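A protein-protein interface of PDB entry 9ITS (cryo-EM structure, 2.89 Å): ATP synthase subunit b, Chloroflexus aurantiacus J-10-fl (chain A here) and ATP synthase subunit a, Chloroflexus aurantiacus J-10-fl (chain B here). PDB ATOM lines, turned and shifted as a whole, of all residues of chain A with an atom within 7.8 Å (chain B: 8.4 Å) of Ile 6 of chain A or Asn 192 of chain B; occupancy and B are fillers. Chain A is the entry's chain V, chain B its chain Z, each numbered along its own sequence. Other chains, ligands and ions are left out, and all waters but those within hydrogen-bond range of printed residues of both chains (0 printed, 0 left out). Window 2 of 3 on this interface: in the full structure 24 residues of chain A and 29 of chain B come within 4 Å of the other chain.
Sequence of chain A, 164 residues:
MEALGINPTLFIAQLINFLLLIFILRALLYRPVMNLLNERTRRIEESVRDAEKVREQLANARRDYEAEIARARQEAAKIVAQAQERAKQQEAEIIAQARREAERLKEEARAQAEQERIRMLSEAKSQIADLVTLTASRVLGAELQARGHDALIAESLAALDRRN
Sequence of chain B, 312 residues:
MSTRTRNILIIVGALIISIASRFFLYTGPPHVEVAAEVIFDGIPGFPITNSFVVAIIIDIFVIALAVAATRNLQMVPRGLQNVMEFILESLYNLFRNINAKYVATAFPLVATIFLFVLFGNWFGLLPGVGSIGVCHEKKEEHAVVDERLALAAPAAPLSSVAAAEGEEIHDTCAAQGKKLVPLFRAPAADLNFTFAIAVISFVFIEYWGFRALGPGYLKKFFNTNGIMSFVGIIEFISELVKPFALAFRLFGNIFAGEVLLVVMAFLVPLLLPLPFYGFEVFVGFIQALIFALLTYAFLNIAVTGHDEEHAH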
ATOM      1  N   GLY A   5       5.896  26.487 -30.396  1.00  0.00           N
ATOM      2  CA  GLY A   5       6.293  25.547 -29.364  1.00  0.00           C
ATOM      3  C   GLY A   5       5.325  25.487 -28.201  1.00  0.00           C
ATOM      4  O   GLY A   5       4.892  26.518 -27.686  1.00  0.00           O
ATOM      5  N   ILE A   6       4.982  24.270 -27.786  1.00  0.00           N
ATOM      6  CA  ILE A   6       4.022  24.062 -26.711  1.00  0.00           C
ATOM      7  C   ILE A   6       4.593  23.235 -25.562  1.00  0.00           C
ATOM      8  O   ILE A   6       4.138  23.398 -24.416  1.00  0.00           O
ATOM      9  CB  ILE A   6       2.729  23.410 -27.254  1.00  0.00           C
ATOM     10  CG1 ILE A   6       2.165  24.228 -28.418  1.00  0.00           C
ATOM     11  CG2 ILE A   6       1.649  23.308 -26.183  1.00  0.00           C
ATOM     12  CD1 ILE A   6       1.074  23.519 -29.189  1.00  0.00           C
ATOM     13  N   ASN A   7       5.599  22.397 -25.806  1.00  0.00           N
ATOM     14  CA  ASN A   7       6.073  21.454 -24.799  1.00  0.00           C
ATOM     15  C   ASN A   7       6.638  22.180 -23.579  1.00  0.00           C
ATOM     16  O   ASN A   7       7.446  23.107 -23.730  1.00  0.00           O
ATOM     17  CB  ASN A   7       7.125  20.521 -25.400  1.00  0.00           C
ATOM     18  CG  ASN A   7       8.180  21.260 -26.206  1.00  0.00           C
ATOM     19  OD1 ASN A   7       8.161  22.487 -26.307  1.00  0.00           O
ATOM     20  ND2 ASN A   7       9.110  20.510 -26.786  1.00  0.00           N
ATOM     21  N   PRO A   8       6.231  21.802 -22.363  1.00  0.00           N
ATOM     22  CA  PRO A   8       6.722  22.516 -21.175  1.00  0.00           C
ATOM     23  C   PRO A   8       8.186  22.261 -20.868  1.00  0.00           C
ATOM     24  O   PRO A   8       8.814  23.100 -20.210  1.00  0.00           O
ATOM     25  CB  PRO A   8       5.814  21.994 -20.049  1.00  0.00           C
ATOM     26  CG  PRO A   8       4.643  21.356 -20.745  1.00  0.00           C
ATOM     27  CD  PRO A   8       5.190  20.819 -22.026  1.00  0.00           C
ATOM     28  N   THR A   9       8.751  21.133 -21.304  1.00  0.00           N
ATOM     29  CA  THR A   9      10.149  20.840 -20.999  1.00  0.00           C
ATOM     30  C   THR A   9      11.084  21.814 -21.707  1.00  0.00           C
ATOM     31  O   THR A   9      12.000  22.372 -21.091  1.00  0.00           O
ATOM     32  CB  THR A   9      10.482  19.399 -21.387  1.00  0.00           C
ATOM     33  OG1 THR A   9      10.319  19.232 -22.800  1.00  0.00           O
ATOM     34  CG2 THR A   9       9.564  18.428 -20.659  1.00  0.00           C
ATOM     35  N   LEU A  10      10.860  22.036 -23.003  1.00  0.00           N
ATOM     36  CA  LEU A  10      11.645  23.016 -23.748  1.00  0.00           C
ATOM     37  C   LEU A  10      11.429  24.421 -23.202  1.00  0.00           C
ATOM     38  O   LEU A  10      12.364  25.231 -23.144  1.00  0.00           O
ATOM     39  CB  LEU A  10      11.268  22.947 -25.227  1.00  0.00           C
ATOM     40  CG  LEU A  10      11.843  23.982 -26.191  1.00  0.00           C
ATOM     41  CD1 LEU A  10      13.361  23.907 -26.237  1.00  0.00           C
ATOM     42  CD2 LEU A  10      11.237  23.776 -27.565  1.00  0.00           C
ATOM     43  N   PHE A  11      10.192  24.726 -22.802  1.00  0.00           N
ATOM     44  CA  PHE A  11       9.873  26.020 -22.208  1.00  0.00           C
ATOM     45  C   PHE A  11      10.677  26.254 -20.934  1.00  0.00           C
ATOM     46  O   PHE A  11      11.282  27.318 -20.749  1.00  0.00           O
ATOM     47  CB  PHE A  11       8.370  26.073 -21.932  1.00  0.00           C
ATOM     48  CG  PHE A  11       7.935  27.243 -21.108  1.00  0.00           C
ATOM     49  CD1 PHE A  11       7.885  28.511 -21.656  1.00  0.00           C
ATOM     50  CD2 PHE A  11       7.556  27.073 -19.787  1.00  0.00           C
ATOM     51  CE1 PHE A  11       7.473  29.585 -20.900  1.00  0.00           C
ATOM     52  CE2 PHE A  11       7.146  28.146 -19.024  1.00  0.00           C
ATOM     53  CZ  PHE A  11       7.106  29.404 -19.582  1.00  0.00           C
ATOM     54  N   ILE A  12      10.714  25.253 -20.052  1.00  0.00           N
ATOM     55  CA  ILE A  12      11.465  25.366 -18.807  1.00  0.00           C
ATOM     56  C   ILE A  12      12.962  25.432 -19.088  1.00  0.00           C
ATOM     57  O   ILE A  12      13.704  26.138 -18.398  1.00  0.00           O
ATOM     58  CB  ILE A  12      11.102  24.203 -17.865  1.00  0.00           C
ATOM     59  CG1 ILE A  12       9.670  24.366 -17.353  1.00  0.00           C
ATOM     60  CG2 ILE A  12      12.066  24.114 -16.689  1.00  0.00           C
ATOM     61  CD1 ILE A  12       9.482  25.547 -16.425  1.00  0.00           C
ATOM     62  N   GLN A  14      14.424  26.786 -21.764  1.00  0.00           N
ATOM     63  CA  GLN A  14      14.716  28.147 -22.205  1.00  0.00           C
ATOM     64  C   GLN A  14      14.617  29.136 -21.048  1.00  0.00           C
ATOM     65  O   GLN A  14      15.405  30.088 -20.962  1.00  0.00           O
ATOM     66  CB  GLN A  14      13.776  28.548 -23.341  1.00  0.00           C
ATOM     67  CG  GLN A  14      14.210  29.799 -24.088  1.00  0.00           C
ATOM     68  CD  GLN A  14      14.975  29.486 -25.360  1.00  0.00           C
ATOM     69  OE1 GLN A  14      14.768  28.445 -25.983  1.00  0.00           O
ATOM     70  NE2 GLN A  14      15.866  30.390 -25.751  1.00  0.00           N
ATOM     71  N   LEU A  15      13.656  28.924 -20.144  1.00  0.00           N
ATOM     72  CA  LEU A  15      13.543  29.776 -18.964  1.00  0.00           C
ATOM     73  C   LEU A  15      14.790  29.682 -18.090  1.00  0.00           C
ATOM     74  O   LEU A  15      15.321  30.704 -17.642  1.00  0.00           O
ATOM     75  CB  LEU A  15      12.289  29.393 -18.175  1.00  0.00           C
ATOM     76  CG  LEU A  15      11.823  30.234 -16.986  1.00  0.00           C
ATOM     77  CD1 LEU A  15      10.310  30.229 -16.927  1.00  0.00           C
ATOM     78  CD2 LEU A  15      12.381  29.686 -15.685  1.00  0.00           C
ATOM     79  N   ALA B  35       5.115  28.646 -38.024  1.00  0.00           N
ATOM     80  CA  ALA B  35       4.804  29.377 -36.805  1.00  0.00           C
ATOM     81  C   ALA B  35       5.326  28.681 -35.556  1.00  0.00           C
ATOM     82  O   ALA B  35       4.940  29.053 -34.444  1.00  0.00           O
ATOM     83  CB  ALA B  35       3.295  29.597 -36.691  1.00  0.00           C
ATOM     84  N   ALA B  36       6.188  27.681 -35.713  1.00  0.00           N
ATOM     85  CA  ALA B  36       6.729  26.935 -34.585  1.00  0.00           C
ATOM     86  C   ALA B  36       8.228  26.761 -34.800  1.00  0.00           C
ATOM     87  O   ALA B  36       8.823  27.365 -35.698  1.00  0.00           O
ATOM     88  CB  ALA B  36       6.004  25.592 -34.422  1.00  0.00           C
ATOM     89  N   GLU B  37       8.841  25.928 -33.967  1.00  0.00           N
ATOM     90  CA  GLU B  37      10.273  25.684 -34.016  1.00  0.00           C
ATOM     91  C   GLU B  37      10.602  24.515 -34.941  1.00  0.00           C
ATOM     92  O   GLU B  37       9.765  23.656 -35.227  1.00  0.00           O
ATOM     93  CB  GLU B  37      10.818  25.402 -32.615  1.00  0.00           C
ATOM     94  CG  GLU B  37      10.062  24.314 -31.863  1.00  0.00           C
ATOM     95  CD  GLU B  37      10.660  22.933 -32.060  1.00  0.00           C
ATOM     96  OE1 GLU B  37      11.846  22.840 -32.438  1.00  0.00           O
ATOM     97  OE2 GLU B  37       9.941  21.937 -31.832  1.00  0.00           O
ATOM     98  N   THR B  49      16.294  23.729 -30.872  1.00  0.00           N
ATOM     99  CA  THR B  49      15.480  24.469 -31.818  1.00  0.00           C
ATOM    100  C   THR B  49      16.350  25.398 -32.660  1.00  0.00           C
ATOM    101  O   THR B  49      17.531  25.620 -32.380  1.00  0.00           O
ATOM    102  CB  THR B  49      14.409  25.280 -31.092  1.00  0.00           C
ATOM    103  OG1 THR B  49      15.033  26.255 -30.249  1.00  0.00           O
ATOM    104  CG2 THR B  49      13.566  24.371 -30.231  1.00  0.00           C
ATOM    105  N   SER B  51      15.785  28.480 -32.694  1.00  0.00           N
ATOM    106  CA  SER B  51      15.907  29.672 -31.869  1.00  0.00           C
ATOM    107  C   SER B  51      16.839  29.473 -30.682  1.00  0.00           C
ATOM    108  O   SER B  51      17.456  30.440 -30.225  1.00  0.00           O
ATOM    109  CB  SER B  51      14.528  30.110 -31.369  1.00  0.00           C
ATOM    110  OG  SER B  51      13.754  30.652 -32.425  1.00  0.00           O
ATOM    111  N   PRO B 187      15.042  34.386 -31.759  1.00  0.00           N
ATOM    112  CA  PRO B 187      14.496  33.808 -30.519  1.00  0.00           C
ATOM    113  C   PRO B 187      13.143  34.371 -30.125  1.00  0.00           C
ATOM    114  O   PRO B 187      12.326  33.638 -29.554  1.00  0.00           O
ATOM    115  CB  PRO B 187      15.570  34.141 -29.475  1.00  0.00           C
ATOM    116  CG  PRO B 187      16.247  35.356 -30.011  1.00  0.00           C
ATOM    117  CD  PRO B 187      16.239  35.209 -31.508  1.00  0.00           C
ATOM    118  N   ALA B 188      12.880  35.647 -30.409  1.00  0.00           N
ATOM    119  CA  ALA B 188      11.589  36.229 -30.071  1.00  0.00           C
ATOM    120  C   ALA B 188      10.470  35.701 -30.957  1.00  0.00           C
ATOM    121  O   ALA B 188       9.305  35.732 -30.547  1.00  0.00           O
ATOM    122  CB  ALA B 188      11.658  37.753 -30.159  1.00  0.00           C
ATOM    123  N   ALA B 189      10.795  35.223 -32.162  1.00  0.00           N
ATOM    124  CA  ALA B 189       9.787  34.587 -33.002  1.00  0.00           C
ATOM    125  C   ALA B 189       9.290  33.288 -32.385  1.00  0.00           C
ATOM    126  O   ALA B 189       8.133  32.906 -32.594  1.00  0.00           O
ATOM    127  CB  ALA B 189      10.350  34.334 -34.400  1.00  0.00           C
ATOM    128  N   ASP B 190      10.146  32.596 -31.640  1.00  0.00           N
ATOM    129  CA  ASP B 190       9.714  31.421 -30.899  1.00  0.00           C
ATOM    130  C   ASP B 190       8.797  31.827 -29.752  1.00  0.00           C
ATOM    131  O   ASP B 190       9.063  32.794 -29.033  1.00  0.00           O
ATOM    132  CB  ASP B 190      10.928  30.662 -30.365  1.00  0.00           C
ATOM    133  CG  ASP B 190      10.544  29.527 -29.443  1.00  0.00           C
ATOM    134  OD1 ASP B 190      10.033  28.500 -29.937  1.00  0.00           O
ATOM    135  OD2 ASP B 190      10.758  29.663 -28.222  1.00  0.00           O
ATOM    136  N   LEU B 191       7.706  31.078 -29.583  1.00  0.00           N
ATOM    137  CA  LEU B 191       6.727  31.413 -28.555  1.00  0.00           C
ATOM    138  C   LEU B 191       7.205  31.055 -27.155  1.00  0.00           C
ATOM    139  O   LEU B 191       6.820  31.724 -26.190  1.00  0.00           O
ATOM    140  CB  LEU B 191       5.398  30.713 -28.844  1.00  0.00           C
ATOM    141  CG  LEU B 191       4.428  31.460 -29.758  1.00  0.00           C
ATOM    142  CD1 LEU B 191       3.378  30.513 -30.314  1.00  0.00           C
ATOM    143  CD2 LEU B 191       3.775  32.611 -29.008  1.00  0.00           C
ATOM    144  N   ASN B 192       8.027  30.010 -27.023  1.00  0.00           N
ATOM    145  CA  ASN B 192       8.457  29.569 -25.699  1.00  0.00           C
ATOM    146  C   ASN B 192       9.307  30.626 -25.006  1.00  0.00           C
ATOM    147  O   ASN B 192       9.148  30.866 -23.806  1.00  0.00           O
ATOM    148  CB  ASN B 192       9.228  28.253 -25.803  1.00  0.00           C
ATOM    149  CG  ASN B 192       8.458  27.185 -26.547  1.00  0.00           C
ATOM    150  OD1 ASN B 192       8.664  26.980 -27.743  1.00  0.00           O
ATOM    151  ND2 ASN B 192       7.565  26.498 -25.846  1.00  0.00           N
ATOM    152  N   PHE B 193      10.214  31.269 -25.747  1.00  0.00           N
ATOM    153  CA  PHE B 193      11.065  32.298 -25.157  1.00  0.00           C
ATOM    154  C   PHE B 193      10.247  33.504 -24.706  1.00  0.00           C
ATOM    155  O   PHE B 193      10.481  34.053 -23.620  1.00  0.00           O
ATOM    156  CB  PHE B 193      12.138  32.716 -26.161  1.00  0.00           C
ATOM    157  CG  PHE B 193      12.721  34.072 -25.898  1.00  0.00           C
ATOM    158  CD1 PHE B 193      13.547  34.285 -24.809  1.00  0.00           C
ATOM    159  CD2 PHE B 193      12.446  35.134 -26.744  1.00  0.00           C
ATOM    160  CE1 PHE B 193      14.086  35.532 -24.568  1.00  0.00           C
ATOM    161  CE2 PHE B 193      12.983  36.383 -26.507  1.00  0.00           C
ATOM    162  CZ  PHE B 193      13.804  36.581 -25.416  1.00  0.00           C
ATOM    163  N   THR B 194       9.289  33.933 -25.531  1.00  0.00           N
ATOM    164  CA  THR B 194       8.434  35.055 -25.158  1.00  0.00           C
ATOM    165  C   THR B 194       7.578  34.718 -23.945  1.00  0.00           C
ATOM    166  O   THR B 194       7.413  35.548 -23.043  1.00  0.00           O
ATOM    167  CB  THR B 194       7.555  35.465 -26.339  1.00  0.00           C
ATOM    168  OG1 THR B 194       6.964  34.298 -26.922  1.00  0.00           O
ATOM    169  CG2 THR B 194       8.384  36.187 -27.391  1.00  0.00           C
ATOM    170  N   PHE B 195       7.032  33.501 -23.899  1.00  0.00           N
ATOM    171  CA  PHE B 195       6.268  33.090 -22.727  1.00  0.00           C
ATOM    172  C   PHE B 195       7.147  33.017 -21.486  1.00  0.00           C
ATOM    173  O   PHE B 195       6.695  33.364 -20.391  1.00  0.00           O
ATOM    174  CB  PHE B 195       5.585  31.747 -22.986  1.00  0.00           C
ATOM    175  CG  PHE B 195       4.270  31.865 -23.700  1.00  0.00           C
ATOM    176  CD1 PHE B 195       3.272  32.688 -23.206  1.00  0.00           C
ATOM    177  CD2 PHE B 195       4.029  31.151 -24.862  1.00  0.00           C
ATOM    178  CE1 PHE B 195       2.059  32.800 -23.860  1.00  0.00           C
ATOM    179  CE2 PHE B 195       2.819  31.258 -25.521  1.00  0.00           C
ATOM    180  CZ  PHE B 195       1.832  32.084 -25.018  1.00  0.00           C
ATOM    181  N   ALA B 196       8.404  32.589 -21.637  1.00  0.00           N
ATOM    182  CA  ALA B 196       9.310  32.513 -20.496  1.00  0.00           C
ATOM    183  C   ALA B 196       9.639  33.895 -19.951  1.00  0.00           C
ATOM    184  O   ALA B 196       9.628  34.104 -18.731  1.00  0.00           O
ATOM    185  CB  ALA B 196      10.587  31.774 -20.890  1.00  0.00           C
ATOM    186  N   ILE B 197       9.937  34.853 -20.831  1.00  0.00           N
ATOM    187  CA  ILE B 197      10.240  36.193 -20.335  1.00  0.00           C
ATOM    188  C   ILE B 197       8.990  36.847 -19.754  1.00  0.00           C
ATOM    189  O   ILE B 197       9.067  37.554 -18.740  1.00  0.00           O
ATOM    190  CB  ILE B 197      10.907  37.057 -21.424  1.00  0.00           C
ATOM    191  CG1 ILE B 197      10.067  37.110 -22.695  1.00  0.00           C
ATOM    192  CG2 ILE B 197      12.301  36.537 -21.723  1.00  0.00           C
ATOM    193  CD1 ILE B 197      10.698  37.904 -23.818  1.00  0.00           C
ATOM    194  N   ALA B 198       7.818  36.596 -20.345  1.00  0.00           N
ATOM    195  CA  ALA B 198       6.584  37.123 -19.774  1.00  0.00           C
ATOM    196  C   ALA B 198       6.310  36.542 -18.391  1.00  0.00           C
ATOM    197  O   ALA B 198       5.928  37.272 -17.469  1.00  0.00           O
ATOM    198  CB  ALA B 198       5.415  36.838 -20.714  1.00  0.00           C
ATOM    199  N   VAL B 199       6.505  35.233 -18.220  1.00  0.00           N
ATOM    200  CA  VAL B 199       6.201  34.620 -16.933  1.00  0.00           C
ATOM    201  C   VAL B 199       7.243  34.992 -15.879  1.00  0.00           C
ATOM    202  O   VAL B 199       6.899  35.133 -14.700  1.00  0.00           O
ATOM    203  CB  VAL B 199       6.032  33.095 -17.079  1.00  0.00           C
ATOM    204  CG1 VAL B 199       7.362  32.392 -17.276  1.00  0.00           C
ATOM    205  CG2 VAL B 199       5.294  32.524 -15.875  1.00  0.00           C
ATOM    206  N   ALA B 247       4.064  38.634 -23.977  1.00  0.00           N
ATOM    207  CA  ALA B 247       4.694  37.655 -24.857  1.00  0.00           C
ATOM    208  C   ALA B 247       4.183  37.784 -26.286  1.00  0.00           C
ATOM    209  O   ALA B 247       4.975  37.741 -27.244  1.00  0.00           O
ATOM    210  CB  ALA B 247       4.447  36.243 -24.329  1.00  0.00           C
ATOM    211  N   PHE B 251       6.248  38.360 -29.879  1.00  0.00           N
ATOM    212  CA  PHE B 251       6.172  37.259 -30.835  1.00  0.00           C
ATOM    213  C   PHE B 251       5.557  37.716 -32.150  1.00  0.00           C
ATOM    214  O   PHE B 251       6.109  37.466 -33.229  1.00  0.00           O
ATOM    215  CB  PHE B 251       5.370  36.101 -30.236  1.00  0.00           C
ATOM    216  CG  PHE B 251       4.687  35.240 -31.262  1.00  0.00           C
ATOM    217  CD1 PHE B 251       5.421  34.385 -32.067  1.00  0.00           C
ATOM    218  CD2 PHE B 251       3.312  35.284 -31.418  1.00  0.00           C
ATOM    219  CE1 PHE B 251       4.797  33.594 -33.011  1.00  0.00           C
ATOM    220  CE2 PHE B 251       2.681  34.493 -32.360  1.00  0.00           C
ATOM    221  CZ  PHE B 251       3.425  33.648 -33.158  1.00  0.00           C
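Hydrophobic or aromatic side chains of chain A within 4 Å of the printed part of chain B: Leu 10, Phe 11 and Leu 15. Hydrophobic or aromatic side chains of chain B within 4 Å of the printed part of chain A: Phe 195, Ala 196 and Val 199. Among the printed residues, 10 pairs touch across the chains. Among the printed residues, no Asp or Glu carboxylate lies within 4 Å of a Lys or Arg side-chain nitrogen of the other chain.
ND2 of Asn 192 of chain B touches N of Ile 6 of chain A, 3.9 Å away. Asn 7 of chain A touches Asn 192 of chain B (O to ND2, 3.999 Å). Thr 49 of chain B touches Leu 10 of chain A (CG2 to CD2, 3.6 Å). Phe 11 of chain A touches Asn 192 of chain B (CD1 to O, 3.4 Å). Phe 11 of chain A touches Phe 195 of chain B. Phe 11 of chain A touches Ala 196 of chain B (CE1 to N, 3.2 Å). Val 199 of chain B touches Phe 11 of chain A. Leu 15 of chain A touches Ala 196 of chain B. Leu 15 of chain A touches Val 199 of chain B.
The side-chain amide nitrogen (ND2) of Asn 192 of chain B sits at hydrogen-bond distance from the backbone carbonyl oxygen (O) of Gly 5 of chain A.
Of chain B, only Asn 192 (3.2 Å) comes within 4 Å of Gly 5 of chain A. Ile 6 of chain A touches just one residue of chain B: Asn 192 (3.9 Å). Printed residues of chain B within 4 Å of Asn 7 of chain A: Asn 192. Of the printed residues of chain B, Phe 11 of chain A touches Asn 192, Phe 195, Ala 196 and Val 199. Printed residues of chain A within 4 Å of Thr 49 of chain B: Leu 10. Asp 190 of chain B touches none of the printed residues of chain A. Leu 191 of chain B touches none of the printed residues of chain A. Printed residues of chain A within 4 Å of Asn 192 of chain B: Gly 5, Ile 6, Asn 7 and Phe 11. Of the printed residues of chain A, Phe 195 of chain B touches Phe 11 (3.5 Å). Of the printed residues of chain A, Ala 196 of chain B touches Phe 11 and Leu 15. The nearest printed residue of chain B that does not touch Ile 6 of chain A is Glu 37 of chain B (6.5 Å).
OG1 of Thr 49 of chain B lies close to N of Ser 51 of chain B (3.4 Å). OD1 of Asp 190 of chain B lies close to OD1 of Asn 192 of chain B (3.0 Å).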
